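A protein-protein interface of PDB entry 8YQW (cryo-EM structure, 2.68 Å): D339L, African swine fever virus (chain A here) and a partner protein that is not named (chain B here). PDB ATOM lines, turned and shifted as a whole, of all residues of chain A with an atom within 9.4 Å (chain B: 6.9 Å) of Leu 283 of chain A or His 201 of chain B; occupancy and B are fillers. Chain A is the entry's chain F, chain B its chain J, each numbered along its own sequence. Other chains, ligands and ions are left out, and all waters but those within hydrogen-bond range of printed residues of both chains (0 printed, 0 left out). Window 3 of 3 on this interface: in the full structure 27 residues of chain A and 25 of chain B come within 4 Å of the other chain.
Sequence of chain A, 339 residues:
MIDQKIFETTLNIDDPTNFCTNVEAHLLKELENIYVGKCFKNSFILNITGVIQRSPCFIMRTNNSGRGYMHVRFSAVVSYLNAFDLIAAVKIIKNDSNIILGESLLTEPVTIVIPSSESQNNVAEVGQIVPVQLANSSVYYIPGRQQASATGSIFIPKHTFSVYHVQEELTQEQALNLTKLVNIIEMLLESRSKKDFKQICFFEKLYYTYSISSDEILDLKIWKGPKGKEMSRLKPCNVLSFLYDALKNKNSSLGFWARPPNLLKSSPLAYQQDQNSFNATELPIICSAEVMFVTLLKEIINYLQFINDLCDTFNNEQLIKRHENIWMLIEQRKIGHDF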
ATOM      1  N   THR A 160     -25.032   2.870   3.115  1.00  0.00           N
ATOM      2  CA  THR A 160     -25.475   4.207   3.469  1.00  0.00           C
ATOM      3  C   THR A 160     -25.107   5.182   2.350  1.00  0.00           C
ATOM      4  O   THR A 160     -24.091   5.033   1.671  1.00  0.00           O
ATOM      5  CB  THR A 160     -24.859   4.622   4.809  1.00  0.00           C
ATOM      6  OG1 THR A 160     -25.268   3.700   5.827  1.00  0.00           O
ATOM      7  CG2 THR A 160     -25.301   6.023   5.211  1.00  0.00           C
ATOM      8  N   PHE A 161     -25.950   6.193   2.161  1.00  0.00           N
ATOM      9  CA  PHE A 161     -25.734   7.198   1.130  1.00  0.00           C
ATOM     10  C   PHE A 161     -25.955   8.572   1.752  1.00  0.00           C
ATOM     11  O   PHE A 161     -26.151   8.700   2.965  1.00  0.00           O
ATOM     12  CB  PHE A 161     -26.655   6.949  -0.072  1.00  0.00           C
ATOM     13  CG  PHE A 161     -28.119   7.061   0.250  1.00  0.00           C
ATOM     14  CD1 PHE A 161     -28.838   5.951   0.657  1.00  0.00           C
ATOM     15  CD2 PHE A 161     -28.780   8.273   0.132  1.00  0.00           C
ATOM     16  CE1 PHE A 161     -30.180   6.049   0.950  1.00  0.00           C
ATOM     17  CE2 PHE A 161     -30.124   8.377   0.425  1.00  0.00           C
ATOM     18  CZ  PHE A 161     -30.824   7.263   0.834  1.00  0.00           C
ATOM     19  N   SER A 162     -25.925   9.607   0.916  1.00  0.00           N
ATOM     20  CA  SER A 162     -26.111  10.974   1.376  1.00  0.00           C
ATOM     21  C   SER A 162     -27.044  11.706   0.425  1.00  0.00           C
ATOM     22  O   SER A 162     -27.142  11.370  -0.758  1.00  0.00           O
ATOM     23  CB  SER A 162     -24.775  11.719   1.481  1.00  0.00           C
ATOM     24  OG  SER A 162     -23.926  11.106   2.435  1.00  0.00           O
ATOM     25  N   VAL A 163     -27.734  12.711   0.958  1.00  0.00           N
ATOM     26  CA  VAL A 163     -28.663  13.535   0.196  1.00  0.00           C
ATOM     27  C   VAL A 163     -28.133  14.960   0.184  1.00  0.00           C
ATOM     28  O   VAL A 163     -27.782  15.507   1.237  1.00  0.00           O
ATOM     29  CB  VAL A 163     -30.083  13.480   0.784  1.00  0.00           C
ATOM     30  CG1 VAL A 163     -31.029  14.341  -0.035  1.00  0.00           C
ATOM     31  CG2 VAL A 163     -30.577  12.047   0.836  1.00  0.00           C
ATOM     32  N   TYR A 164     -28.067  15.556  -1.001  1.00  0.00           N
ATOM     33  CA  TYR A 164     -27.590  16.921  -1.174  1.00  0.00           C
ATOM     34  C   TYR A 164     -28.771  17.816  -1.523  1.00  0.00           C
ATOM     35  O   TYR A 164     -29.458  17.584  -2.523  1.00  0.00           O
ATOM     36  CB  TYR A 164     -26.512  16.990  -2.256  1.00  0.00           C
ATOM     37  CG  TYR A 164     -25.266  16.213  -1.908  1.00  0.00           C
ATOM     38  CD1 TYR A 164     -24.314  16.739  -1.048  1.00  0.00           C
ATOM     39  CD2 TYR A 164     -25.045  14.946  -2.431  1.00  0.00           C
ATOM     40  CE1 TYR A 164     -23.177  16.030  -0.721  1.00  0.00           C
ATOM     41  CE2 TYR A 164     -23.912  14.229  -2.111  1.00  0.00           C
ATOM     42  CZ  TYR A 164     -22.981  14.776  -1.256  1.00  0.00           C
ATOM     43  OH  TYR A 164     -21.850  14.063  -0.934  1.00  0.00           O
ATOM     44  N   HIS A 165     -29.008  18.825  -0.693  1.00  0.00           N
ATOM     45  CA  HIS A 165     -30.074  19.792  -0.914  1.00  0.00           C
ATOM     46  C   HIS A 165     -29.480  21.002  -1.625  1.00  0.00           C
ATOM     47  O   HIS A 165     -28.733  21.782  -1.022  1.00  0.00           O
ATOM     48  CB  HIS A 165     -30.722  20.183   0.409  1.00  0.00           C
ATOM     49  CG  HIS A 165     -31.958  21.012   0.256  1.00  0.00           C
ATOM     50  ND1 HIS A 165     -33.070  20.571  -0.429  1.00  0.00           N
ATOM     51  CD2 HIS A 165     -32.262  22.249   0.711  1.00  0.00           C
ATOM     52  CE1 HIS A 165     -34.002  21.506  -0.396  1.00  0.00           C
ATOM     53  NE2 HIS A 165     -33.538  22.534   0.290  1.00  0.00           N
ATOM     54  N   PHE A 256     -33.625  17.972  -3.979  1.00  0.00           N
ATOM     55  CA  PHE A 256     -32.979  16.913  -3.212  1.00  0.00           C
ATOM     56  C   PHE A 256     -32.365  15.914  -4.187  1.00  0.00           C
ATOM     57  O   PHE A 256     -33.086  15.202  -4.894  1.00  0.00           O
ATOM     58  CB  PHE A 256     -33.979  16.234  -2.281  1.00  0.00           C
ATOM     59  CG  PHE A 256     -34.430  17.101  -1.141  1.00  0.00           C
ATOM     60  CD1 PHE A 256     -33.729  17.120   0.051  1.00  0.00           C
ATOM     61  CD2 PHE A 256     -35.555  17.898  -1.264  1.00  0.00           C
ATOM     62  CE1 PHE A 256     -34.141  17.919   1.102  1.00  0.00           C
ATOM     63  CE2 PHE A 256     -35.974  18.701  -0.216  1.00  0.00           C
ATOM     64  CZ  PHE A 256     -35.266  18.710   0.968  1.00  0.00           C
ATOM     65  N   ASN A 276     -37.786  15.695  -0.230  1.00  0.00           N
ATOM     66  CA  ASN A 276     -36.881  14.722   0.377  1.00  0.00           C
ATOM     67  C   ASN A 276     -37.636  13.410   0.565  1.00  0.00           C
ATOM     68  O   ASN A 276     -38.049  13.037   1.666  1.00  0.00           O
ATOM     69  CB  ASN A 276     -36.329  15.246   1.696  1.00  0.00           C
ATOM     70  CG  ASN A 276     -35.204  14.387   2.238  1.00  0.00           C
ATOM     71  OD1 ASN A 276     -34.696  13.500   1.550  1.00  0.00           O
ATOM     72  ND2 ASN A 276     -34.811  14.645   3.479  1.00  0.00           N
ATOM     73  N   PHE A 278     -36.208  10.563  -0.084  1.00  0.00           N
ATOM     74  CA  PHE A 278     -35.208   9.539   0.171  1.00  0.00           C
ATOM     75  C   PHE A 278     -35.227   9.135   1.638  1.00  0.00           C
ATOM     76  O   PHE A 278     -35.428   9.969   2.525  1.00  0.00           O
ATOM     77  CB  PHE A 278     -33.818  10.046  -0.215  1.00  0.00           C
ATOM     78  CG  PHE A 278     -33.780  10.748  -1.540  1.00  0.00           C
ATOM     79  CD1 PHE A 278     -33.779  10.026  -2.721  1.00  0.00           C
ATOM     80  CD2 PHE A 278     -33.757  12.130  -1.605  1.00  0.00           C
ATOM     81  CE1 PHE A 278     -33.747  10.669  -3.940  1.00  0.00           C
ATOM     82  CE2 PHE A 278     -33.726  12.778  -2.822  1.00  0.00           C
ATOM     83  CZ  PHE A 278     -33.720  12.046  -3.991  1.00  0.00           C
ATOM     84  N   ASN A 279     -35.020   7.845   1.889  1.00  0.00           N
ATOM     85  CA  ASN A 279     -35.001   7.315   3.252  1.00  0.00           C
ATOM     86  C   ASN A 279     -33.596   7.431   3.845  1.00  0.00           C
ATOM     87  O   ASN A 279     -32.963   6.452   4.241  1.00  0.00           O
ATOM     88  CB  ASN A 279     -35.498   5.874   3.262  1.00  0.00           C
ATOM     89  CG  ASN A 279     -36.874   5.732   2.643  1.00  0.00           C
ATOM     90  OD1 ASN A 279     -37.045   5.051   1.631  1.00  0.00           O
ATOM     91  ND2 ASN A 279     -37.864   6.381   3.245  1.00  0.00           N
ATOM     92  N   ALA A 280     -33.115   8.670   3.896  1.00  0.00           N
ATOM     93  CA  ALA A 280     -31.777   8.939   4.398  1.00  0.00           C
ATOM     94  C   ALA A 280     -31.728   8.800   5.915  1.00  0.00           C
ATOM     95  O   ALA A 280     -32.682   9.127   6.626  1.00  0.00           O
ATOM     96  CB  ALA A 280     -31.325  10.338   3.987  1.00  0.00           C
ATOM     97  N   THR A 281     -30.592   8.308   6.408  1.00  0.00           N
ATOM     98  CA  THR A 281     -30.357   8.149   7.836  1.00  0.00           C
ATOM     99  C   THR A 281     -29.535   9.294   8.416  1.00  0.00           C
ATOM    100  O   THR A 281     -28.907   9.129   9.467  1.00  0.00           O
ATOM    101  CB  THR A 281     -29.670   6.812   8.114  1.00  0.00           C
ATOM    102  OG1 THR A 281     -28.353   6.823   7.549  1.00  0.00           O
ATOM    103  CG2 THR A 281     -30.468   5.669   7.506  1.00  0.00           C
ATOM    104  N   GLU A 282     -29.525  10.445   7.749  1.00  0.00           N
ATOM    105  CA  GLU A 282     -28.785  11.606   8.222  1.00  0.00           C
ATOM    106  C   GLU A 282     -29.418  12.856   7.630  1.00  0.00           C
ATOM    107  O   GLU A 282     -30.173  12.790   6.657  1.00  0.00           O
ATOM    108  CB  GLU A 282     -27.299  11.519   7.852  1.00  0.00           C
ATOM    109  CG  GLU A 282     -26.983  11.915   6.418  1.00  0.00           C
ATOM    110  CD  GLU A 282     -27.552  10.947   5.396  1.00  0.00           C
ATOM    111  OE1 GLU A 282     -27.896   9.807   5.775  1.00  0.00           O
ATOM    112  OE2 GLU A 282     -27.659  11.327   4.212  1.00  0.00           O
ATOM    113  N   LEU A 283     -29.101  13.993   8.234  1.00  0.00           N
ATOM    114  CA  LEU A 283     -29.676  15.259   7.793  1.00  0.00           C
ATOM    115  C   LEU A 283     -29.168  15.608   6.399  1.00  0.00           C
ATOM    116  O   LEU A 283     -27.963  15.499   6.139  1.00  0.00           O
ATOM    117  CB  LEU A 283     -29.331  16.376   8.774  1.00  0.00           C
ATOM    118  CG  LEU A 283     -30.232  16.535  10.002  1.00  0.00           C
ATOM    119  CD1 LEU A 283     -30.024  15.402  10.996  1.00  0.00           C
ATOM    120  CD2 LEU A 283     -29.991  17.884  10.665  1.00  0.00           C
ATOM    121  N   PRO A 284     -30.047  16.008   5.474  1.00  0.00           N
ATOM    122  CA  PRO A 284     -29.587  16.421   4.142  1.00  0.00           C
ATOM    123  C   PRO A 284     -28.575  17.551   4.207  1.00  0.00           C
ATOM    124  O   PRO A 284     -28.683  18.449   5.046  1.00  0.00           O
ATOM    125  CB  PRO A 284     -30.876  16.869   3.438  1.00  0.00           C
ATOM    126  CG  PRO A 284     -32.017  16.440   4.323  1.00  0.00           C
ATOM    127  CD  PRO A 284     -31.480  15.675   5.485  1.00  0.00           C
ATOM    128  N   ILE A 285     -27.585  17.508   3.322  1.00  0.00           N
ATOM    129  CA  ILE A 285     -26.488  18.465   3.324  1.00  0.00           C
ATOM    130  C   ILE A 285     -26.867  19.642   2.437  1.00  0.00           C
ATOM    131  O   ILE A 285     -26.993  19.492   1.218  1.00  0.00           O
ATOM    132  CB  ILE A 285     -25.187  17.811   2.838  1.00  0.00           C
ATOM    133  CG1 ILE A 285     -24.892  16.548   3.649  1.00  0.00           C
ATOM    134  CG2 ILE A 285     -24.034  18.794   2.908  1.00  0.00           C
ATOM    135  CD1 ILE A 285     -24.067  15.526   2.903  1.00  0.00           C
ATOM    136  N   ILE A 286     -27.052  20.813   3.046  1.00  0.00           N
ATOM    137  CA  ILE A 286     -27.367  22.010   2.277  1.00  0.00           C
ATOM    138  C   ILE A 286     -26.119  22.470   1.540  1.00  0.00           C
ATOM    139  O   ILE A 286     -25.049  22.633   2.142  1.00  0.00           O
ATOM    140  CB  ILE A 286     -27.907  23.116   3.196  1.00  0.00           C
ATOM    141  CG1 ILE A 286     -28.945  22.553   4.169  1.00  0.00           C
ATOM    142  CG2 ILE A 286     -28.501  24.249   2.374  1.00  0.00           C
ATOM    143  CD1 ILE A 286     -30.167  21.973   3.501  1.00  0.00           C
ATOM    144  N   CYS A 287     -26.242  22.684   0.233  1.00  0.00           N
ATOM    145  CA  CYS A 287     -25.098  23.090  -0.574  1.00  0.00           C
ATOM    146  C   CYS A 287     -25.606  23.732  -1.858  1.00  0.00           C
ATOM    147  O   CYS A 287     -26.795  24.026  -2.002  1.00  0.00           O
ATOM    148  CB  CYS A 287     -24.184  21.899  -0.872  1.00  0.00           C
ATOM    149  SG  CYS A 287     -24.895  20.680  -2.002  1.00  0.00           S
ATOM    150  N   GLU B  76     -23.557  16.074  21.954  1.00  0.00           N
ATOM    151  CA  GLU B  76     -23.337  17.395  21.381  1.00  0.00           C
ATOM    152  C   GLU B  76     -22.054  18.028  21.904  1.00  0.00           C
ATOM    153  O   GLU B  76     -21.439  18.843  21.206  1.00  0.00           O
ATOM    154  CB  GLU B  76     -24.539  18.297  21.666  1.00  0.00           C
ATOM    155  CG  GLU B  76     -24.472  19.653  20.986  1.00  0.00           C
ATOM    156  CD  GLU B  76     -24.520  19.552  19.476  1.00  0.00           C
ATOM    157  OE1 GLU B  76     -25.143  18.601  18.962  1.00  0.00           O
ATOM    158  OE2 GLU B  76     -23.928  20.421  18.803  1.00  0.00           O
ATOM    159  N   ILE B  79     -18.999  17.260  19.585  1.00  0.00           N
ATOM    160  CA  ILE B  79     -18.993  18.000  18.327  1.00  0.00           C
ATOM    161  C   ILE B  79     -18.699  19.475  18.573  1.00  0.00           C
ATOM    162  O   ILE B  79     -17.845  20.076  17.907  1.00  0.00           O
ATOM    163  CB  ILE B  79     -20.330  17.801  17.589  1.00  0.00           C
ATOM    164  CG1 ILE B  79     -20.497  16.337  17.177  1.00  0.00           C
ATOM    165  CG2 ILE B  79     -20.403  18.699  16.373  1.00  0.00           C
ATOM    166  CD1 ILE B  79     -21.880  15.999  16.668  1.00  0.00           C
ATOM    167  N   LEU B  83     -15.479  21.657  17.122  1.00  0.00           N
ATOM    168  CA  LEU B  83     -15.607  22.843  16.280  1.00  0.00           C
ATOM    169  C   LEU B  83     -14.867  24.056  16.833  1.00  0.00           C
ATOM    170  O   LEU B  83     -14.595  24.992  16.076  1.00  0.00           O
ATOM    171  CB  LEU B  83     -17.082  23.192  16.082  1.00  0.00           C
ATOM    172  CG  LEU B  83     -17.731  22.647  14.808  1.00  0.00           C
ATOM    173  CD1 LEU B  83     -17.892  21.136  14.867  1.00  0.00           C
ATOM    174  CD2 LEU B  83     -19.064  23.330  14.554  1.00  0.00           C
ATOM    175  N   PHE B 172     -22.131  26.311   1.792  1.00  0.00           N
ATOM    176  CA  PHE B 172     -22.458  25.297   2.790  1.00  0.00           C
ATOM    177  C   PHE B 172     -23.196  25.916   3.970  1.00  0.00           C
ATOM    178  O   PHE B 172     -24.125  25.315   4.522  1.00  0.00           O
ATOM    179  CB  PHE B 172     -21.188  24.590   3.264  1.00  0.00           C
ATOM    180  CG  PHE B 172     -20.905  23.305   2.546  1.00  0.00           C
ATOM    181  CD1 PHE B 172     -21.442  22.114   3.000  1.00  0.00           C
ATOM    182  CD2 PHE B 172     -20.101  23.285   1.422  1.00  0.00           C
ATOM    183  CE1 PHE B 172     -21.183  20.929   2.344  1.00  0.00           C
ATOM    184  CE2 PHE B 172     -19.839  22.102   0.763  1.00  0.00           C
ATOM    185  CZ  PHE B 172     -20.382  20.923   1.224  1.00  0.00           C
ATOM    186  N   GLU B 194     -31.697  23.928  18.128  1.00  0.00           N
ATOM    187  CA  GLU B 194     -31.756  23.156  16.889  1.00  0.00           C
ATOM    188  C   GLU B 194     -30.762  23.678  15.860  1.00  0.00           C
ATOM    189  O   GLU B 194     -30.075  22.895  15.186  1.00  0.00           O
ATOM    190  CB  GLU B 194     -33.171  23.206  16.313  1.00  0.00           C
ATOM    191  CG  GLU B 194     -34.250  22.633  17.214  1.00  0.00           C
ATOM    192  CD  GLU B 194     -35.646  22.923  16.697  1.00  0.00           C
ATOM    193  OE1 GLU B 194     -35.771  23.719  15.742  1.00  0.00           O
ATOM    194  OE2 GLU B 194     -36.617  22.361  17.244  1.00  0.00           O
ATOM    195  N   ASN B 195     -30.673  24.999  15.723  1.00  0.00           N
ATOM    196  CA  ASN B 195     -29.829  25.566  14.685  1.00  0.00           C
ATOM    197  C   ASN B 195     -28.348  25.475  15.024  1.00  0.00           C
ATOM    198  O   ASN B 195     -27.526  25.504  14.108  1.00  0.00           O
ATOM    199  CB  ASN B 195     -30.244  27.008  14.414  1.00  0.00           C
ATOM    200  CG  ASN B 195     -31.454  27.096  13.506  1.00  0.00           C
ATOM    201  OD1 ASN B 195     -32.414  27.811  13.796  1.00  0.00           O
ATOM    202  ND2 ASN B 195     -31.411  26.374  12.392  1.00  0.00           N
ATOM    203  N   ILE B 196     -27.982  25.353  16.302  1.00  0.00           N
ATOM    204  CA  ILE B 196     -26.597  25.016  16.620  1.00  0.00           C
ATOM    205  C   ILE B 196     -26.258  23.631  16.086  1.00  0.00           C
ATOM    206  O   ILE B 196     -25.171  23.407  15.540  1.00  0.00           O
ATOM    207  CB  ILE B 196     -26.335  25.123  18.134  1.00  0.00           C
ATOM    208  CG1 ILE B 196     -26.024  26.568  18.523  1.00  0.00           C
ATOM    209  CG2 ILE B 196     -25.196  24.206  18.560  1.00  0.00           C
ATOM    210  CD1 ILE B 196     -25.853  26.775  20.012  1.00  0.00           C
ATOM    211  N   ILE B 197     -27.186  22.683  16.225  1.00  0.00           N
ATOM    212  CA  ILE B 197     -26.980  21.354  15.656  1.00  0.00           C
ATOM    213  C   ILE B 197     -26.854  21.443  14.141  1.00  0.00           C
ATOM    214  O   ILE B 197     -25.983  20.804  13.536  1.00  0.00           O
ATOM    215  CB  ILE B 197     -28.124  20.413  16.080  1.00  0.00           C
ATOM    216  CG1 ILE B 197     -28.061  20.139  17.583  1.00  0.00           C
ATOM    217  CG2 ILE B 197     -28.062  19.112  15.299  1.00  0.00           C
ATOM    218  CD1 ILE B 197     -29.324  19.527  18.148  1.00  0.00           C
ATOM    219  N   GLN B 198     -27.713  22.246  13.506  1.00  0.00           N
ATOM    220  CA  GLN B 198     -27.621  22.423  12.058  1.00  0.00           C
ATOM    221  C   GLN B 198     -26.284  23.040  11.655  1.00  0.00           C
ATOM    222  O   GLN B 198     -25.676  22.629  10.660  1.00  0.00           O
ATOM    223  CB  GLN B 198     -28.779  23.287  11.559  1.00  0.00           C
ATOM    224  CG  GLN B 198     -28.917  23.321  10.048  1.00  0.00           C
ATOM    225  CD  GLN B 198     -29.932  24.343   9.579  1.00  0.00           C
ATOM    226  OE1 GLN B 198     -30.454  25.127  10.373  1.00  0.00           O
ATOM    227  NE2 GLN B 198     -30.221  24.340   8.283  1.00  0.00           N
ATOM    228  N   PHE B 199     -25.820  24.038  12.412  1.00  0.00           N
ATOM    229  CA  PHE B 199     -24.548  24.691  12.123  1.00  0.00           C
ATOM    230  C   PHE B 199     -23.385  23.720  12.255  1.00  0.00           C
ATOM    231  O   PHE B 199     -22.473  23.716  11.421  1.00  0.00           O
ATOM    232  CB  PHE B 199     -24.373  25.888  13.062  1.00  0.00           C
ATOM    233  CG  PHE B 199     -23.047  26.586  12.941  1.00  0.00           C
ATOM    234  CD1 PHE B 199     -21.968  26.199  13.721  1.00  0.00           C
ATOM    235  CD2 PHE B 199     -22.887  27.645  12.067  1.00  0.00           C
ATOM    236  CE1 PHE B 199     -20.753  26.848  13.619  1.00  0.00           C
ATOM    237  CE2 PHE B 199     -21.673  28.299  11.960  1.00  0.00           C
ATOM    238  CZ  PHE B 199     -20.605  27.899  12.738  1.00  0.00           C
ATOM    239  N   THR B 200     -23.394  22.896  13.304  1.00  0.00           N
ATOM    240  CA  THR B 200     -22.343  21.899  13.470  1.00  0.00           C
ATOM    241  C   THR B 200     -22.363  20.886  12.334  1.00  0.00           C
ATOM    242  O   THR B 200     -21.307  20.506  11.808  1.00  0.00           O
ATOM    243  CB  THR B 200     -22.499  21.198  14.818  1.00  0.00           C
ATOM    244  OG1 THR B 200     -23.840  20.713  14.951  1.00  0.00           O
ATOM    245  CG2 THR B 200     -22.201  22.160  15.955  1.00  0.00           C
ATOM    246  N   HIS B 201     -23.558  20.442  11.937  1.00  0.00           N
ATOM    247  CA  HIS B 201     -23.670  19.510  10.820  1.00  0.00           C
ATOM    248  C   HIS B 201     -23.132  20.123   9.534  1.00  0.00           C
ATOM    249  O   HIS B 201     -22.412  19.463   8.775  1.00  0.00           O
ATOM    250  CB  HIS B 201     -25.128  19.081  10.651  1.00  0.00           C
ATOM    251  CG  HIS B 201     -25.391  18.304   9.400  1.00  0.00           C
ATOM    252  ND1 HIS B 201     -25.968  18.868   8.282  1.00  0.00           N
ATOM    253  CD2 HIS B 201     -25.159  17.008   9.088  1.00  0.00           C
ATOM    254  CE1 HIS B 201     -26.080  17.952   7.337  1.00  0.00           C
ATOM    255  NE2 HIS B 201     -25.595  16.815   7.801  1.00  0.00           N
ATOM    256  N   GLN B 202     -23.457  21.392   9.280  1.00  0.00           N
ATOM    257  CA  GLN B 202     -22.993  22.041   8.058  1.00  0.00           C
ATOM    258  C   GLN B 202     -21.486  22.265   8.084  1.00  0.00           C
ATOM    259  O   GLN B 202     -20.822  22.140   7.053  1.00  0.00           O
ATOM    260  CB  GLN B 202     -23.737  23.357   7.847  1.00  0.00           C
ATOM    261  CG  GLN B 202     -25.187  23.176   7.417  1.00  0.00           C
ATOM    262  CD  GLN B 202     -25.335  22.227   6.243  1.00  0.00           C
ATOM    263  OE1 GLN B 202     -25.973  21.180   6.354  1.00  0.00           O
ATOM    264  NE2 GLN B 202     -24.741  22.586   5.111  1.00  0.00           N
ATOM    265  N   TYR B 203     -20.929  22.597   9.252  1.00  0.00           N
ATOM    266  CA  TYR B 203     -19.478  22.701   9.390  1.00  0.00           C
ATOM    267  C   TYR B 203     -18.798  21.372   9.081  1.00  0.00           C
ATOM    268  O   TYR B 203     -17.813  21.321   8.325  1.00  0.00           O
ATOM    269  CB  TYR B 203     -19.139  23.156  10.810  1.00  0.00           C
ATOM    270  CG  TYR B 203     -17.764  23.755  10.997  1.00  0.00           C
ATOM    271  CD1 TYR B 203     -17.536  25.101  10.765  1.00  0.00           C
ATOM    272  CD2 TYR B 203     -16.704  22.981  11.440  1.00  0.00           C
ATOM    273  CE1 TYR B 203     -16.288  25.656  10.946  1.00  0.00           C
ATOM    274  CE2 TYR B 203     -15.453  23.527  11.629  1.00  0.00           C
ATOM    275  CZ  TYR B 203     -15.250  24.866  11.379  1.00  0.00           C
ATOM    276  OH  TYR B 203     -14.003  25.419  11.560  1.00  0.00           O
ATOM    277  N   ILE B 204     -19.317  20.286   9.660  1.00  0.00           N
ATOM    278  CA  ILE B 204     -18.748  18.963   9.421  1.00  0.00           C
ATOM    279  C   ILE B 204     -18.807  18.625   7.940  1.00  0.00           C
ATOM    280  O   ILE B 204     -17.826  18.157   7.352  1.00  0.00           O
ATOM    281  CB  ILE B 204     -19.472  17.904  10.273  1.00  0.00           C
ATOM    282  CG1 ILE B 204     -19.074  18.035  11.744  1.00  0.00           C
ATOM    283  CG2 ILE B 204     -19.171  16.501   9.761  1.00  0.00           C
ATOM    284  CD1 ILE B 204     -17.604  17.808  12.001  1.00  0.00           C
ATOM    285  N   GLU B 205     -19.956  18.875   7.307  1.00  0.00           N
ATOM    286  CA  GLU B 205     -20.100  18.552   5.893  1.00  0.00           C
ATOM    287  C   GLU B 205     -19.197  19.419   5.023  1.00  0.00           C
ATOM    288  O   GLU B 205     -18.639  18.940   4.031  1.00  0.00           O
ATOM    289  CB  GLU B 205     -21.559  18.696   5.467  1.00  0.00           C
ATOM    290  CG  GLU B 205     -22.501  17.735   6.171  1.00  0.00           C
ATOM    291  CD  GLU B 205     -22.110  16.283   5.984  1.00  0.00           C
ATOM    292  OE1 GLU B 205     -21.555  15.940   4.919  1.00  0.00           O
ATOM    293  OE2 GLU B 205     -22.357  15.481   6.908  1.00  0.00           O
ATOM    294  N   LEU B 206     -19.033  20.696   5.379  1.00  0.00           N
ATOM    295  CA  LEU B 206     -18.187  21.582   4.590  1.00  0.00           C
ATOM    296  C   LEU B 206     -16.736  21.125   4.620  1.00  0.00           C
ATOM    297  O   LEU B 206     -16.081  21.031   3.576  1.00  0.00           O
ATOM    298  CB  LEU B 206     -18.310  23.018   5.103  1.00  0.00           C
ATOM    299  CG  LEU B 206     -17.155  23.963   4.766  1.00  0.00           C
ATOM    300  CD1 LEU B 206     -17.189  24.359   3.298  1.00  0.00           C
ATOM    301  CD2 LEU B 206     -17.195  25.192   5.654  1.00  0.00           C
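Among the printed residues, merely in contact across the chains: Ile 285 of chain A with Glu 205 of chain B, Pro 284 of chain A with His 201 of chain B, Ile 285 of chain A with Phe 172 of chain B and Ile 286 of chain A with Phe 172 of chain B.
Of chain B, only His 201 comes within 4 Å of Leu 283 of chain A. Gln 202 of chain B touches just one residue of chain A: Ile 286 (3.0 Å). Of the printed residues of chain B, Pro 284 of chain A touches His 201. Of the printed residues of chain A, Phe 172 of chain B touches Ile 285 and Ile 286. Of the printed residues of chain B, Ile 286 of chain A touches Phe 172 and Gln 202. Phe 278 of chain A touches none of the printed residues of chain B. The nearest residue of chain B that does not touch Leu 283 of chain A is Ile 197 of chain B (5.2 Å). The nearest printed residue of chain B that does not touch Ile 285 of chain A is His 201 of chain B (4.1 Å).
The backbone carbonyl oxygen (O) of Phe 172 of chain B lies within hydrogen-bond range of the side-chain amide nitrogen (NE2) of Gln 202 of chain B, 2.9 Å away. O of Val 163 of chain A lies within hydrogen-bond range of N of Ile 285 of chain A (2.9 Å). The backbone carbonyl oxygen (O) of Ile 285 of chain A is in hydrogen-bond range of the backbone NH (N) of His 165 of chain A (2.9 Å). A ring nitrogen (ND1) of His 201 of chain B is in hydrogen-bond range of the side-chain amide oxygen (OE1) of Gln 202 of chain B (3.0 Å).
O of Leu 283 of chain A is in hydrogen-bond range of NE2 of His 201 of chain B (3.2 Å). The side-chain amide nitrogen (NE2) of Gln 202 of chain B lies within hydrogen-bond range of the backbone carbonyl oxygen (O) of Ile 286 of chain A.
Of the 18 printed residues of chain A, 4 touch a printed residue of chain B. Hydrophobic or aromatic side chains of chain A that line the printed part of chain B: Leu 283, Ile 285 and Ile 286. Among the printed residues, 6 pairs touch across the chains.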
